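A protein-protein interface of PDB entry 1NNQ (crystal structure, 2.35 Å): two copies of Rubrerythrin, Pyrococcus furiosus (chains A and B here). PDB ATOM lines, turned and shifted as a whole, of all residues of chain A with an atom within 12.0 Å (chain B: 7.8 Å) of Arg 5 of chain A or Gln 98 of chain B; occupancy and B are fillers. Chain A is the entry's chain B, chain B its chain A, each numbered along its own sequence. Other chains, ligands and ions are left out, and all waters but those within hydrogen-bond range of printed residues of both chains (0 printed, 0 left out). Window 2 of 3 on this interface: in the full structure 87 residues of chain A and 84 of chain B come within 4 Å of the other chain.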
ATOM      1  N   VAL A   2      11.520 -22.531   5.203  1.00  0.00           N
ATOM      2  CA  VAL A   2      12.710 -21.610   5.113  1.00  0.00           C
ATOM      3  C   VAL A   2      13.717 -21.971   6.203  1.00  0.00           C
ATOM      4  O   VAL A   2      13.388 -21.992   7.400  1.00  0.00           O
ATOM      5  CB  VAL A   2      12.333 -20.106   5.211  1.00  0.00           C
ATOM      6  CG1 VAL A   2      13.568 -19.227   5.385  1.00  0.00           C
ATOM      7  CG2 VAL A   2      11.552 -19.664   3.985  1.00  0.00           C
ATOM      8  N   VAL A   3      14.938 -22.250   5.754  1.00  0.00           N
ATOM      9  CA  VAL A   3      16.020 -22.774   6.575  1.00  0.00           C
ATOM     10  C   VAL A   3      16.454 -21.766   7.621  1.00  0.00           C
ATOM     11  O   VAL A   3      16.745 -20.625   7.289  1.00  0.00           O
ATOM     12  CB  VAL A   3      17.220 -23.162   5.657  1.00  0.00           C
ATOM     13  CG1 VAL A   3      18.411 -23.684   6.462  1.00  0.00           C
ATOM     14  CG2 VAL A   3      16.741 -24.206   4.637  1.00  0.00           C
ATOM     15  N   LYS A   4      16.515 -22.209   8.876  1.00  0.00           N
ATOM     16  CA  LYS A   4      16.863 -21.334   9.996  1.00  0.00           C
ATOM     17  C   LYS A   4      18.117 -21.796  10.749  1.00  0.00           C
ATOM     18  O   LYS A   4      18.885 -20.964  11.235  1.00  0.00           O
ATOM     19  CB  LYS A   4      15.671 -21.204  10.977  1.00  0.00           C
ATOM     20  CG  LYS A   4      14.373 -20.563  10.378  1.00  0.00           C
ATOM     21  N   ARG A   5      18.337 -23.101  10.857  1.00  0.00           N
ATOM     22  CA  ARG A   5      19.521 -23.594  11.564  1.00  0.00           C
ATOM     23  C   ARG A   5      20.811 -23.019  10.961  1.00  0.00           C
ATOM     24  O   ARG A   5      21.020 -23.073   9.739  1.00  0.00           O
ATOM     25  CB  ARG A   5      19.561 -25.124  11.561  1.00  0.00           C
ATOM     26  CG  ARG A   5      18.366 -25.813  12.237  1.00  0.00           C
ATOM     27  CD  ARG A   5      18.170 -25.498  13.711  1.00  0.00           C
ATOM     28  NE  ARG A   5      19.359 -25.769  14.525  1.00  0.00           N
ATOM     29  CZ  ARG A   5      19.641 -26.939  15.111  1.00  0.00           C
ATOM     30  NH1 ARG A   5      20.744 -27.059  15.848  1.00  0.00           N
ATOM     31  NH2 ARG A   5      18.832 -27.991  14.964  1.00  0.00           N
ATOM     32  N   THR A   6      21.673 -22.465  11.813  1.00  0.00           N
ATOM     33  CA  THR A   6      22.896 -21.788  11.362  1.00  0.00           C
ATOM     34  C   THR A   6      23.735 -22.650  10.398  1.00  0.00           C
ATOM     35  O   THR A   6      24.147 -22.166   9.363  1.00  0.00           O
ATOM     36  CB  THR A   6      23.764 -21.366  12.568  1.00  0.00           C
ATOM     37  OG1 THR A   6      22.975 -20.603  13.476  1.00  0.00           O
ATOM     38  CG2 THR A   6      24.869 -20.371  12.165  1.00  0.00           C
ATOM     39  N   MET A   7      24.006 -23.899  10.751  1.00  0.00           N
ATOM     40  CA  MET A   7      24.926 -24.729   9.936  1.00  0.00           C
ATOM     41  C   MET A   7      24.358 -25.036   8.553  1.00  0.00           C
ATOM     42  O   MET A   7      25.032 -24.804   7.553  1.00  0.00           O
ATOM     43  CB  MET A   7      25.329 -26.035  10.644  1.00  0.00           C
ATOM     44  CG  MET A   7      26.183 -25.842  11.910  1.00  0.00           C
ATOM     45  SD  MET A   7      27.619 -24.740  11.773  1.00  0.00           S
ATOM     46  CE  MET A   7      28.820 -25.776  10.889  1.00  0.00           C
ATOM     47  N   THR A   8      23.117 -25.529   8.505  1.00  0.00           N
ATOM     48  CA  THR A   8      22.465 -25.889   7.254  1.00  0.00           C
ATOM     49  C   THR A   8      22.356 -24.686   6.306  1.00  0.00           C
ATOM     50  O   THR A   8      22.572 -24.813   5.096  1.00  0.00           O
ATOM     51  CB  THR A   8      21.071 -26.499   7.537  1.00  0.00           C
ATOM     52  OG1 THR A   8      21.226 -27.790   8.151  1.00  0.00           O
ATOM     53  CG2 THR A   8      20.354 -26.811   6.250  1.00  0.00           C
ATOM     54  N   LYS A   9      22.037 -23.532   6.877  1.00  0.00           N
ATOM     55  CA  LYS A   9      21.925 -22.269   6.161  1.00  0.00           C
ATOM     56  C   LYS A   9      23.251 -21.880   5.518  1.00  0.00           C
ATOM     57  O   LYS A   9      23.308 -21.569   4.309  1.00  0.00           O
ATOM     58  CB  LYS A   9      21.486 -21.178   7.141  1.00  0.00           C
ATOM     59  CG  LYS A   9      21.400 -19.790   6.581  1.00  0.00           C
ATOM     60  CD  LYS A   9      20.845 -18.824   7.651  1.00  0.00           C
ATOM     61  CE  LYS A   9      20.689 -17.415   7.094  1.00  0.00           C
ATOM     62  N   LYS A  10      24.305 -21.899   6.324  1.00  0.00           N
ATOM     63  CA  LYS A  10      25.652 -21.654   5.836  1.00  0.00           C
ATOM     64  C   LYS A  10      26.026 -22.666   4.718  1.00  0.00           C
ATOM     65  O   LYS A  10      26.588 -22.274   3.707  1.00  0.00           O
ATOM     66  CB  LYS A  10      26.619 -21.667   7.008  1.00  0.00           C
ATOM     67  CG  LYS A  10      28.065 -21.938   6.703  1.00  0.00           C
ATOM     68  CD  LYS A  10      28.986 -21.374   7.825  1.00  0.00           C
ATOM     69  CE  LYS A  10      28.793 -22.081   9.179  1.00  0.00           C
ATOM     70  NZ  LYS A  10      29.716 -21.483  10.196  1.00  0.00           N
ATOM     71  N   PHE A  11      25.644 -23.926   4.874  1.00  0.00           N
ATOM     72  CA  PHE A  11      25.888 -24.949   3.851  1.00  0.00           C
ATOM     73  C   PHE A  11      25.125 -24.668   2.542  1.00  0.00           C
ATOM     74  O   PHE A  11      25.706 -24.775   1.451  1.00  0.00           O
ATOM     75  CB  PHE A  11      25.542 -26.353   4.370  1.00  0.00           C
ATOM     76  CG  PHE A  11      26.461 -26.843   5.457  1.00  0.00           C
ATOM     77  CD1 PHE A  11      26.160 -28.005   6.165  1.00  0.00           C
ATOM     78  CD2 PHE A  11      27.641 -26.175   5.746  1.00  0.00           C
ATOM     79  CE1 PHE A  11      26.992 -28.465   7.145  1.00  0.00           C
ATOM     80  CE2 PHE A  11      28.487 -26.648   6.745  1.00  0.00           C
ATOM     81  CZ  PHE A  11      28.153 -27.797   7.446  1.00  0.00           C
ATOM     82  N   LEU A  12      23.844 -24.314   2.661  1.00  0.00           N
ATOM     83  CA  LEU A  12      23.062 -23.923   1.496  1.00  0.00           C
ATOM     84  C   LEU A  12      23.659 -22.706   0.785  1.00  0.00           C
ATOM     85  O   LEU A  12      23.675 -22.674  -0.437  1.00  0.00           O
ATOM     86  CB  LEU A  12      21.613 -23.622   1.872  1.00  0.00           C
ATOM     87  CG  LEU A  12      20.618 -24.780   1.956  1.00  0.00           C
ATOM     88  CD1 LEU A  12      19.200 -24.239   1.809  1.00  0.00           C
ATOM     89  CD2 LEU A  12      20.876 -25.895   0.938  1.00  0.00           C
ATOM     90  N   GLU A  13      24.137 -21.721   1.562  1.00  0.00           N
ATOM     91  CA  GLU A  13      24.761 -20.527   1.022  1.00  0.00           C
ATOM     92  C   GLU A  13      26.012 -20.922   0.222  1.00  0.00           C
ATOM     93  O   GLU A  13      26.277 -20.363  -0.839  1.00  0.00           O
ATOM     94  CB  GLU A  13      25.072 -19.501   2.145  1.00  0.00           C
ATOM     95  CG  GLU A  13      23.920 -18.508   2.372  1.00  0.00           C
ATOM     96  CD  GLU A  13      23.826 -17.876   3.768  1.00  0.00           C
ATOM     97  OE1 GLU A  13      22.847 -17.112   3.994  1.00  0.00           O
ATOM     98  OE2 GLU A  13      24.700 -18.093   4.649  1.00  0.00           O
ATOM     99  N   GLU A  14      26.756 -21.908   0.715  1.00  0.00           N
ATOM    100  CA  GLU A  14      27.955 -22.378   0.036  1.00  0.00           C
ATOM    101  C   GLU A  14      27.584 -23.146  -1.227  1.00  0.00           C
ATOM    102  O   GLU A  14      28.209 -22.971  -2.289  1.00  0.00           O
ATOM    103  CB  GLU A  14      28.807 -23.228   0.965  1.00  0.00           C
ATOM    104  CG  GLU A  14      30.136 -23.659   0.351  1.00  0.00           C
ATOM    105  CD  GLU A  14      31.029 -22.471  -0.045  1.00  0.00           C
ATOM    106  OE1 GLU A  14      31.032 -21.416   0.661  1.00  0.00           O
ATOM    107  OE2 GLU A  14      31.730 -22.597  -1.070  1.00  0.00           O
ATOM    108  N   HIS A  59      18.085 -23.745  -3.846  1.00  0.00           N
ATOM    109  CA  HIS A  59      18.778 -23.388  -2.610  1.00  0.00           C
ATOM    110  C   HIS A  59      18.370 -21.979  -2.204  1.00  0.00           C
ATOM    111  O   HIS A  59      18.114 -21.741  -1.039  1.00  0.00           O
ATOM    112  CB  HIS A  59      20.295 -23.423  -2.765  1.00  0.00           C
ATOM    113  CG  HIS A  59      20.847 -24.767  -3.094  1.00  0.00           C
ATOM    114  ND1 HIS A  59      20.341 -25.939  -2.566  1.00  0.00           N
ATOM    115  CD2 HIS A  59      21.891 -25.125  -3.878  1.00  0.00           C
ATOM    116  CE1 HIS A  59      21.032 -26.962  -3.036  1.00  0.00           C
ATOM    117  NE2 HIS A  59      21.979 -26.497  -3.832  1.00  0.00           N
ATOM    118  N   ALA A  62      14.851 -21.944  -0.866  1.00  0.00           N
ATOM    119  CA  ALA A  62      14.928 -22.557   0.466  1.00  0.00           C
ATOM    120  C   ALA A  62      15.565 -21.650   1.523  1.00  0.00           C
ATOM    121  O   ALA A  62      15.220 -21.747   2.696  1.00  0.00           O
ATOM    122  CB  ALA A  62      15.646 -23.860   0.415  1.00  0.00           C
ATOM    123  N   LEU A  63      16.495 -20.792   1.111  1.00  0.00           N
ATOM    124  CA  LEU A  63      17.084 -19.783   1.995  1.00  0.00           C
ATOM    125  C   LEU A  63      16.174 -18.572   2.270  1.00  0.00           C
ATOM    126  O   LEU A  63      16.513 -17.707   3.065  1.00  0.00           O
ATOM    127  CB  LEU A  63      18.420 -19.298   1.436  1.00  0.00           C
ATOM    128  CG  LEU A  63      19.636 -20.197   1.711  1.00  0.00           C
ATOM    129  CD1 LEU A  63      20.786 -19.850   0.741  1.00  0.00           C
ATOM    130  CD2 LEU A  63      20.086 -20.088   3.165  1.00  0.00           C
ATOM    131  N   GLY A  64      15.026 -18.516   1.607  1.00  0.00           N
ATOM    132  CA  GLY A  64      14.078 -17.435   1.824  1.00  0.00           C
ATOM    133  C   GLY A  64      14.490 -16.146   1.145  1.00  0.00           C
ATOM    134  O   GLY A  64      14.069 -15.081   1.573  1.00  0.00           O
ATOM    135  N   LYS A  65      15.298 -16.241   0.084  1.00  0.00           N
ATOM    136  CA  LYS A  65      15.944 -15.064  -0.490  1.00  0.00           C
ATOM    137  C   LYS A  65      15.195 -14.434  -1.668  1.00  0.00           C
ATOM    138  O   LYS A  65      15.587 -13.391  -2.174  1.00  0.00           O
ATOM    139  CB  LYS A  65      17.384 -15.396  -0.883  1.00  0.00           C
ATOM    140  CG  LYS A  65      18.356 -15.244   0.278  1.00  0.00           C
ATOM    141  CD  LYS A  65      19.756 -15.707  -0.105  1.00  0.00           C
ATOM    142  CE  LYS A  65      20.657 -15.839   1.126  1.00  0.00           C
ATOM    143  NZ  LYS A  65      21.078 -14.508   1.639  1.00  0.00           N
ATOM    144  N   TYR B  91      26.188 -32.288   3.218  1.00  0.00           N
ATOM    145  CA  TYR B  91      25.204 -31.210   3.415  1.00  0.00           C
ATOM    146  C   TYR B  91      23.825 -31.814   3.627  1.00  0.00           C
ATOM    147  O   TYR B  91      23.077 -31.364   4.474  1.00  0.00           O
ATOM    148  CB  TYR B  91      25.166 -30.263   2.193  1.00  0.00           C
ATOM    149  CG  TYR B  91      26.312 -29.269   2.102  1.00  0.00           C
ATOM    150  CD1 TYR B  91      27.321 -29.251   3.059  1.00  0.00           C
ATOM    151  CD2 TYR B  91      26.397 -28.358   1.036  1.00  0.00           C
ATOM    152  CE1 TYR B  91      28.356 -28.332   2.990  1.00  0.00           C
ATOM    153  CE2 TYR B  91      27.450 -27.446   0.951  1.00  0.00           C
ATOM    154  CZ  TYR B  91      28.400 -27.443   1.931  1.00  0.00           C
ATOM    155  OH  TYR B  91      29.428 -26.571   1.899  1.00  0.00           O
ATOM    156  N   ASN B  92      23.514 -32.850   2.843  1.00  0.00           N
ATOM    157  CA  ASN B  92      22.259 -33.577   2.938  1.00  0.00           C
ATOM    158  C   ASN B  92      22.095 -34.189   4.325  1.00  0.00           C
ATOM    159  O   ASN B  92      21.055 -34.024   4.946  1.00  0.00           O
ATOM    160  CB  ASN B  92      22.190 -34.661   1.847  1.00  0.00           C
ATOM    161  CG  ASN B  92      20.928 -35.494   1.919  1.00  0.00           C
ATOM    162  OD1 ASN B  92      20.915 -36.567   2.513  1.00  0.00           O
ATOM    163  ND2 ASN B  92      19.858 -34.997   1.325  1.00  0.00           N
ATOM    164  N   LYS B  93      23.130 -34.875   4.808  1.00  0.00           N
ATOM    165  CA  LYS B  93      23.122 -35.463   6.146  1.00  0.00           C
ATOM    166  C   LYS B  93      23.001 -34.437   7.298  1.00  0.00           C
ATOM    167  O   LYS B  93      22.357 -34.706   8.308  1.00  0.00           O
ATOM    168  CB  LYS B  93      24.354 -36.340   6.349  1.00  0.00           C
ATOM    169  CG  LYS B  93      24.192 -37.431   7.431  1.00  0.00           C
ATOM    170  N   ALA B  94      23.616 -33.268   7.146  1.00  0.00           N
ATOM    171  CA  ALA B  94      23.555 -32.244   8.183  1.00  0.00           C
ATOM    172  C   ALA B  94      22.161 -31.652   8.196  1.00  0.00           C
ATOM    173  O   ALA B  94      21.582 -31.408   9.280  1.00  0.00           O
ATOM    174  CB  ALA B  94      24.601 -31.150   7.923  1.00  0.00           C
ATOM    175  N   ALA B  95      21.619 -31.413   7.002  1.00  0.00           N
ATOM    176  CA  ALA B  95      20.242 -30.957   6.866  1.00  0.00           C
ATOM    177  C   ALA B  95      19.293 -31.909   7.592  1.00  0.00           C
ATOM    178  O   ALA B  95      18.445 -31.471   8.353  1.00  0.00           O
ATOM    179  CB  ALA B  95      19.841 -30.831   5.389  1.00  0.00           C
ATOM    180  N   GLU B  96      19.442 -33.207   7.347  1.00  0.00           N
ATOM    181  CA  GLU B  96      18.583 -34.217   7.958  1.00  0.00           C
ATOM    182  C   GLU B  96      18.808 -34.219   9.464  1.00  0.00           C
ATOM    183  O   GLU B  96      17.853 -34.192  10.241  1.00  0.00           O
ATOM    184  CB  GLU B  96      18.814 -35.591   7.300  1.00  0.00           C
ATOM    185  CG  GLU B  96      18.480 -36.830   8.140  1.00  0.00           C
ATOM    186  CD  GLU B  96      19.244 -38.076   7.684  1.00  0.00           C
ATOM    187  OE1 GLU B  96      19.431 -38.279   6.460  1.00  0.00           O
ATOM    188  OE2 GLU B  96      19.685 -38.853   8.555  1.00  0.00           O
ATOM    189  N   PHE B  97      20.075 -34.162   9.868  1.00  0.00           N
ATOM    190  CA  PHE B  97      20.418 -34.161  11.286  1.00  0.00           C
ATOM    191  C   PHE B  97      19.836 -32.914  11.992  1.00  0.00           C
ATOM    192  O   PHE B  97      19.514 -32.958  13.173  1.00  0.00           O
ATOM    193  CB  PHE B  97      21.938 -34.265  11.453  1.00  0.00           C
ATOM    194  CG  PHE B  97      22.431 -33.985  12.844  1.00  0.00           C
ATOM    195  CD1 PHE B  97      23.045 -32.765  13.143  1.00  0.00           C
ATOM    196  CD2 PHE B  97      22.318 -34.958  13.853  1.00  0.00           C
ATOM    197  CE1 PHE B  97      23.532 -32.492  14.428  1.00  0.00           C
ATOM    198  CE2 PHE B  97      22.784 -34.700  15.175  1.00  0.00           C
ATOM    199  CZ  PHE B  97      23.402 -33.454  15.452  1.00  0.00           C
ATOM    200  N   GLN B  98      19.693 -31.817  11.247  1.00  0.00           N
ATOM    201  CA  GLN B  98      19.230 -30.554  11.826  1.00  0.00           C
ATOM    202  C   GLN B  98      17.718 -30.349  11.653  1.00  0.00           C
ATOM    203  O   GLN B  98      17.209 -29.279  11.962  1.00  0.00           O
ATOM    204  CB  GLN B  98      20.018 -29.370  11.235  1.00  0.00           C
ATOM    205  CG  GLN B  98      21.428 -29.255  11.811  1.00  0.00           C
ATOM    206  CD  GLN B  98      21.989 -27.857  11.726  1.00  0.00           C
ATOM    207  OE1 GLN B  98      21.958 -27.249  10.662  1.00  0.00           O
ATOM    208  NE2 GLN B  98      22.515 -27.339  12.844  1.00  0.00           N
ATOM    209  N   GLY B  99      17.028 -31.372  11.136  1.00  0.00           N
ATOM    210  CA  GLY B  99      15.597 -31.332  10.888  1.00  0.00           C
ATOM    211  C   GLY B  99      15.153 -30.328   9.832  1.00  0.00           C
ATOM    212  O   GLY B  99      13.986 -29.930   9.839  1.00  0.00           O
ATOM    213  N   GLU B 100      16.044 -29.948   8.910  1.00  0.00           N
ATOM    214  CA  GLU B 100      15.758 -28.938   7.876  1.00  0.00           C
ATOM    215  C   GLU B 100      15.293 -29.583   6.559  1.00  0.00           C
ATOM    216  O   GLU B 100      16.077 -29.776   5.591  1.00  0.00           O
ATOM    217  CB  GLU B 100      16.974 -28.025   7.659  1.00  0.00           C
ATOM    218  CG  GLU B 100      17.257 -27.071   8.821  1.00  0.00           C
ATOM    219  CD  GLU B 100      16.283 -25.893   8.871  1.00  0.00           C
ATOM    220  OE1 GLU B 100      16.489 -24.967   9.701  1.00  0.00           O
ATOM    221  OE2 GLU B 100      15.298 -25.886   8.088  1.00  0.00           O
ATOM    222  N   LYS B 101      14.000 -29.893   6.529  1.00  0.00           N
ATOM    223  CA  LYS B 101      13.419 -30.766   5.517  1.00  0.00           C
ATOM    224  C   LYS B 101      13.544 -30.199   4.109  1.00  0.00           C
ATOM    225  O   LYS B 101      13.697 -30.952   3.144  1.00  0.00           O
ATOM    226  CB  LYS B 101      11.947 -31.073   5.847  1.00  0.00           C
ATOM    227  N   VAL B 104      16.996 -30.799   3.026  1.00  0.00           N
ATOM    228  CA  VAL B 104      17.130 -32.227   2.706  1.00  0.00           C
ATOM    229  C   VAL B 104      16.651 -32.434   1.259  1.00  0.00           C
ATOM    230  O   VAL B 104      17.296 -33.151   0.456  1.00  0.00           O
ATOM    231  CB  VAL B 104      16.319 -33.149   3.675  1.00  0.00           C
ATOM    232  CG1 VAL B 104      16.172 -34.612   3.134  1.00  0.00           C
ATOM    233  CG2 VAL B 104      16.933 -33.163   5.069  1.00  0.00           C
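NH1 of Arg 5 of chain A sits close to NE2 of Gln 98 of chain B (3.5 Å).
OE1 of Gln 98 of chain B lies within hydrogen-bond range of OG1 of Thr 8 of chain A (2.7 Å).
The backbone NH (N) of Lys 4 of chain A lies within hydrogen-bond range of the side-chain carboxylate (OE1) of Glu 100 of chain B (2.9 Å).
The backbone NH (N) of Arg 5 of chain A lies within hydrogen-bond range of the side-chain carboxylate (OE1) of Glu 100 of chain B (2.9 Å).
N of Glu 100 of chain B is in hydrogen-bond range of O of Ala 95 of chain B, at 2.9 Å.
N of Val 3 of chain A lies within hydrogen-bond range of O of Ala 62 of chain A, 3.1 Å away.
OE2 of Glu 100 of chain B touches CA of Val 3 of chain A, 3.5 Å away.
Gln 98 of chain B touches Met 7 of chain A.
Ala 94 of chain B touches Thr 8 of chain A (O to OG1, 3.8 Å).
Thr 8 of chain A touches Ala 95 of chain B.
Thr 8 of chain A touches Glu 100 of chain B (CG2 to CB, 3.9 Å).
Phe 11 of chain A touches Tyr 91 of chain B.
Ala 94 of chain B touches Phe 11 of chain A.
CG of Glu 14 of chain A touches OH of Tyr 91 of chain B (3.4 Å).
Gln 98 of chain B touches just these residues of chain A: Arg 5, Met 7 and Thr 8.
Ala 94 of chain B touches just these residues of chain A: Thr 8 and Phe 11.
No residue of chain A comes within 4 Å of Phe 97 of chain B.
No residue of chain A comes within 4 Å of Gly 99 of chain B.
Of the printed residues of chain A, Tyr 91 of chain B touches Phe 11 (3.2 Å) and Glu 14 (3.4 Å).
Of the printed residues of chain B, Glu 14 of chain A touches Tyr 91 (3.4 Å).
Glu 13 of chain A touches none of the printed residues of chain B.
The nearest residue of chain A that does not touch Gln 98 of chain B is Thr 6 of chain A (4.9 Å).
Of the 18 printed residues of chain A, 7 touch a printed residue of chain B.
Hydrophobic or aromatic side chains of chain A that line the printed part of chain B: Val 3, Met 7 and Phe 11.
Of the 12 printed residues of chain B, 5 touch a printed residue of chain A.
Hydrophobic or aromatic side chains of chain B within 4 Å of the printed part of chain A: Tyr 91 and Ala 94.
Among the printed residues, no Asp or Glu carboxylate lies within 4 Å of a Lys or Arg side-chain nitrogen of the other chain.
No position is printed for both chains.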
